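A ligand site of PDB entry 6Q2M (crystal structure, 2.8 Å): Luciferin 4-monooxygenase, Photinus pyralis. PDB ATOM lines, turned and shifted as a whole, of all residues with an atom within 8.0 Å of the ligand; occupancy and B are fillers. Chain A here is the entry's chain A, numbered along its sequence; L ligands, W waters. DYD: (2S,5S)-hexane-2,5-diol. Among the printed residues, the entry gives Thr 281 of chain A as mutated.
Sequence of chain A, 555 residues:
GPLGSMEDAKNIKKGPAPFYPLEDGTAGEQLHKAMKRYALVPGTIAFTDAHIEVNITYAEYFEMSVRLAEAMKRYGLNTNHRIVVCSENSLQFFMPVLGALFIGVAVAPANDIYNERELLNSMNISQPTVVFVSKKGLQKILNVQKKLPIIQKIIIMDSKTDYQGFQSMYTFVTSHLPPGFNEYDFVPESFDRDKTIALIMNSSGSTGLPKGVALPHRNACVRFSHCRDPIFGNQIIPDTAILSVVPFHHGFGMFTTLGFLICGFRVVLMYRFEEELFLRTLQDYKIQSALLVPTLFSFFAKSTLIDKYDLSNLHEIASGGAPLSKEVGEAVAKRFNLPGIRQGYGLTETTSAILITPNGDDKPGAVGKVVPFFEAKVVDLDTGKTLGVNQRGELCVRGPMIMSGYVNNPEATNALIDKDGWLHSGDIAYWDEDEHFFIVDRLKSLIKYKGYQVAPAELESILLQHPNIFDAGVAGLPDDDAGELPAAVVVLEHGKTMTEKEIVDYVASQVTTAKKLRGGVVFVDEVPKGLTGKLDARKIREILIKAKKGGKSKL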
ATOM      1  N   ILE A  45     -18.825  23.449   4.060  1.00  0.00           N
ATOM      2  CA  ILE A  45     -18.618  23.332   2.615  1.00  0.00           C
ATOM      3  C   ILE A  45     -18.635  21.860   2.263  1.00  0.00           C
ATOM      4  O   ILE A  45     -17.936  21.065   2.892  1.00  0.00           O
ATOM      5  CB  ILE A  45     -17.301  24.020   2.191  1.00  0.00           C
ATOM      6  CG1 ILE A  45     -17.313  25.484   2.602  1.00  0.00           C
ATOM      7  CG2 ILE A  45     -17.083  23.890   0.684  1.00  0.00           C
ATOM      8  CD1 ILE A  45     -16.026  26.219   2.348  1.00  0.00           C
ATOM      9  N   THR A  48     -15.463  21.479  -3.059  1.00  0.00           N
ATOM     10  CA  THR A  48     -14.601  22.569  -3.480  1.00  0.00           C
ATOM     11  C   THR A  48     -13.858  22.138  -4.748  1.00  0.00           C
ATOM     12  O   THR A  48     -13.114  21.156  -4.713  1.00  0.00           O
ATOM     13  CB  THR A  48     -13.590  22.950  -2.395  1.00  0.00           C
ATOM     14  OG1 THR A  48     -14.260  23.510  -1.262  1.00  0.00           O
ATOM     15  CG2 THR A  48     -12.576  23.952  -2.934  1.00  0.00           C
ATOM     16  N   ALA A  50     -10.829  22.615  -6.649  1.00  0.00           N
ATOM     17  CA  ALA A  50      -9.558  23.239  -6.320  1.00  0.00           C
ATOM     18  C   ALA A  50      -8.938  23.971  -7.505  1.00  0.00           C
ATOM     19  O   ALA A  50      -8.101  24.864  -7.308  1.00  0.00           O
ATOM     20  CB  ALA A  50      -8.590  22.192  -5.787  1.00  0.00           C
ATOM     21  N   GLU A  53     -11.279  27.177  -7.740  1.00  0.00           N
ATOM     22  CA  GLU A  53     -11.495  27.758  -6.424  1.00  0.00           C
ATOM     23  C   GLU A  53     -12.946  28.229  -6.244  1.00  0.00           C
ATOM     24  O   GLU A  53     -13.210  29.393  -5.942  1.00  0.00           O
ATOM     25  CB  GLU A  53     -10.500  28.898  -6.182  1.00  0.00           C
ATOM     26  CG  GLU A  53      -9.044  28.456  -6.108  1.00  0.00           C
ATOM     27  CD  GLU A  53      -8.087  29.572  -5.739  1.00  0.00           C
ATOM     28  OE1 GLU A  53      -8.552  30.730  -5.583  1.00  0.00           O
ATOM     29  OE2 GLU A  53      -6.872  29.301  -5.613  1.00  0.00           O
ATOM     30  N   VAL A  54     -13.873  27.308  -6.445  1.00  0.00           N
ATOM     31  CA  VAL A  54     -15.295  27.546  -6.210  1.00  0.00           C
ATOM     32  C   VAL A  54     -15.766  26.572  -5.137  1.00  0.00           C
ATOM     33  O   VAL A  54     -15.396  25.389  -5.153  1.00  0.00           O
ATOM     34  CB  VAL A  54     -16.144  27.366  -7.494  1.00  0.00           C
ATOM     35  CG1 VAL A  54     -17.615  27.561  -7.171  1.00  0.00           C
ATOM     36  CG2 VAL A  54     -15.692  28.325  -8.586  1.00  0.00           C
ATOM     37  N   ASN A  55     -16.533  27.074  -4.176  1.00  0.00           N
ATOM     38  CA  ASN A  55     -17.073  26.257  -3.113  1.00  0.00           C
ATOM     39  C   ASN A  55     -18.583  26.113  -3.259  1.00  0.00           C
ATOM     40  O   ASN A  55     -19.264  27.010  -3.765  1.00  0.00           O
ATOM     41  CB  ASN A  55     -16.753  26.864  -1.749  1.00  0.00           C
ATOM     42  CG  ASN A  55     -15.284  26.827  -1.440  1.00  0.00           C
ATOM     43  OD1 ASN A  55     -14.601  25.858  -1.774  1.00  0.00           O
ATOM     44  ND2 ASN A  55     -14.777  27.888  -0.825  1.00  0.00           N
ATOM     45  N   ARG A 266     -15.439  18.138   3.884  1.00  0.00           N
ATOM     46  CA  ARG A 266     -15.270  19.012   2.732  1.00  0.00           C
ATOM     47  C   ARG A 266     -14.480  18.232   1.677  1.00  0.00           C
ATOM     48  O   ARG A 266     -13.319  17.885   1.890  1.00  0.00           O
ATOM     49  CB  ARG A 266     -14.531  20.287   3.134  1.00  0.00           C
ATOM     50  CG  ARG A 266     -14.387  21.290   2.010  1.00  0.00           C
ATOM     51  CD  ARG A 266     -13.624  22.522   2.445  1.00  0.00           C
ATOM     52  NE  ARG A 266     -13.535  23.498   1.353  1.00  0.00           N
ATOM     53  CZ  ARG A 266     -12.914  24.671   1.446  1.00  0.00           C
ATOM     54  NH1 ARG A 266     -12.321  25.027   2.583  1.00  0.00           N
ATOM     55  NH2 ARG A 266     -12.894  25.491   0.409  1.00  0.00           N
ATOM     56  N   ARG A 280       0.119  22.500  -3.399  1.00  0.00           N
ATOM     57  CA  ARG A 280      -0.576  23.733  -3.075  1.00  0.00           C
ATOM     58  C   ARG A 280      -1.969  23.443  -2.514  1.00  0.00           C
ATOM     59  O   ARG A 280      -2.398  24.072  -1.546  1.00  0.00           O
ATOM     60  CB  ARG A 280      -0.710  24.617  -4.323  1.00  0.00           C
ATOM     61  CG  ARG A 280       0.271  25.772  -4.369  1.00  0.00           C
ATOM     62  CD  ARG A 280      -0.130  26.832  -5.401  1.00  0.00           C
ATOM     63  NE  ARG A 280      -0.020  26.365  -6.777  1.00  0.00           N
ATOM     64  CZ  ARG A 280      -1.010  26.385  -7.649  1.00  0.00           C
ATOM     65  NH1 ARG A 280      -2.205  26.872  -7.293  1.00  0.00           N
ATOM     66  NH2 ARG A 280      -0.827  25.934  -8.887  1.00  0.00           N
ATOM     67  N   THR A 281      -2.668  22.478  -3.102  1.00  0.00           N
ATOM     68  CA  THR A 281      -4.022  22.186  -2.647  1.00  0.00           C
ATOM     69  C   THR A 281      -4.000  21.606  -1.256  1.00  0.00           C
ATOM     70  O   THR A 281      -4.786  22.012  -0.391  1.00  0.00           O
ATOM     71  CB  THR A 281      -4.683  21.241  -3.645  1.00  0.00           C
ATOM     72  OG1 THR A 281      -4.659  21.836  -4.942  1.00  0.00           O
ATOM     73  CG2 THR A 281      -6.131  21.009  -3.259  1.00  0.00           C
ATOM     74  N   GLN A 283      -1.870  22.226   0.980  1.00  0.00           N
ATOM     75  CA  GLN A 283      -1.529  23.291   1.921  1.00  0.00           C
ATOM     76  C   GLN A 283      -2.696  24.239   2.128  1.00  0.00           C
ATOM     77  O   GLN A 283      -3.124  24.486   3.264  1.00  0.00           O
ATOM     78  CB  GLN A 283      -0.323  24.086   1.416  1.00  0.00           C
ATOM     79  CG  GLN A 283       0.204  25.099   2.435  1.00  0.00           C
ATOM     80  CD  GLN A 283       1.281  26.024   1.859  1.00  0.00           C
ATOM     81  OE1 GLN A 283       1.498  26.076   0.651  1.00  0.00           O
ATOM     82  NE2 GLN A 283       1.977  26.727   2.739  1.00  0.00           N
ATOM     83  N   ASP A 284      -3.248  24.760   1.031  1.00  0.00           N
ATOM     84  CA  ASP A 284      -4.169  25.890   1.107  1.00  0.00           C
ATOM     85  C   ASP A 284      -5.540  25.494   1.650  1.00  0.00           C
ATOM     86  O   ASP A 284      -6.228  26.326   2.240  1.00  0.00           O
ATOM     87  CB  ASP A 284      -4.296  26.537  -0.275  1.00  0.00           C
ATOM     88  CG  ASP A 284      -2.993  27.214  -0.697  1.00  0.00           C
ATOM     89  OD1 ASP A 284      -2.118  27.414   0.176  1.00  0.00           O
ATOM     90  OD2 ASP A 284      -2.872  27.604  -1.885  1.00  0.00           O
ATOM     91  N   TYR A 285      -5.960  24.245   1.445  1.00  0.00           N
ATOM     92  CA  TYR A 285      -7.234  23.793   1.984  1.00  0.00           C
ATOM     93  C   TYR A 285      -7.079  22.989   3.258  1.00  0.00           C
ATOM     94  O   TYR A 285      -8.071  22.477   3.773  1.00  0.00           O
ATOM     95  CB  TYR A 285      -7.995  22.983   0.929  1.00  0.00           C
ATOM     96  CG  TYR A 285      -8.400  23.856  -0.242  1.00  0.00           C
ATOM     97  CD1 TYR A 285      -9.453  24.737  -0.137  1.00  0.00           C
ATOM     98  CD2 TYR A 285      -7.734  23.772  -1.455  1.00  0.00           C
ATOM     99  CE1 TYR A 285      -9.827  25.534  -1.202  1.00  0.00           C
ATOM    100  CE2 TYR A 285      -8.107  24.550  -2.516  1.00  0.00           C
ATOM    101  CZ  TYR A 285      -9.154  25.436  -2.390  1.00  0.00           C
ATOM    102  OH  TYR A 285      -9.535  26.225  -3.446  1.00  0.00           O
ATOM    103  N   LYS A 286      -5.859  22.883   3.782  1.00  0.00           N
ATOM    104  CA  LYS A 286      -5.611  22.173   5.039  1.00  0.00           C
ATOM    105  C   LYS A 286      -6.121  20.735   4.975  1.00  0.00           C
ATOM    106  O   LYS A 286      -6.893  20.283   5.813  1.00  0.00           O
ATOM    107  CB  LYS A 286      -6.226  22.941   6.214  1.00  0.00           C
ATOM    108  CG  LYS A 286      -5.615  24.307   6.386  1.00  0.00           C
ATOM    109  CD  LYS A 286      -5.955  24.926   7.724  1.00  0.00           C
ATOM    110  CE  LYS A 286      -5.250  26.271   7.912  1.00  0.00           C
ATOM    111  NZ  LYS A 286      -3.770  26.128   8.115  1.00  0.00           N
HETATM  112  C01 DYD L   1      -7.220  30.165  -1.717  1.00  0.00           C
HETATM  113  C02 DYD L   1      -7.580  29.338  -0.483  1.00  0.00           C
HETATM  114  C03 DYD L   1      -9.023  29.597  -0.065  1.00  0.00           C
HETATM  115  C04 DYD L   1      -9.534  28.464   0.826  1.00  0.00           C
HETATM  116  C05 DYD L   1     -10.900  28.883   1.378  1.00  0.00           C
HETATM  117  C06 DYD L   1     -11.237  28.120   2.656  1.00  0.00           C
HETATM  118  O07 DYD L   1     -11.905  28.657   0.424  1.00  0.00           O
HETATM  119  O08 DYD L   1      -7.437  27.995  -0.814  1.00  0.00           O
HETATM  120  O   HOH W   1      -9.096  26.509   4.498  1.00  0.00           O
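The side-chain amide oxygen of Asn 55 sits at hydrogen-bond distance from the guanidinium group of Arg 266 (2.8 Å).
The side-chain amide oxygen (OD1) of Asn 55 is in hydrogen-bond range of the side-chain hydroxyl (OG1) of Thr 48.
The side-chain hydroxyl of Thr 48 sits at hydrogen-bond distance from the guanidinium group of Arg 266, at 2.7 Å.
O07 of the ligand sits at hydrogen-bond distance from ND2 of Asn 55 (3.2 Å).
The guanidinium group (NH2) of Arg 266 is in hydrogen-bond range of an oxygen (O07) of the ligand, at 3.3 Å.
Residues that only touch the ligand: Asp 284 and Tyr 285.
Hydrophobic or aromatic side chains within 4 Å of the ligand: Tyr 285.
Of the 13 residues printed, 4 come within 4 Å of the ligand.
The nearest printed residue that does not touch the ligand is Glu 53 (4.01 Å).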
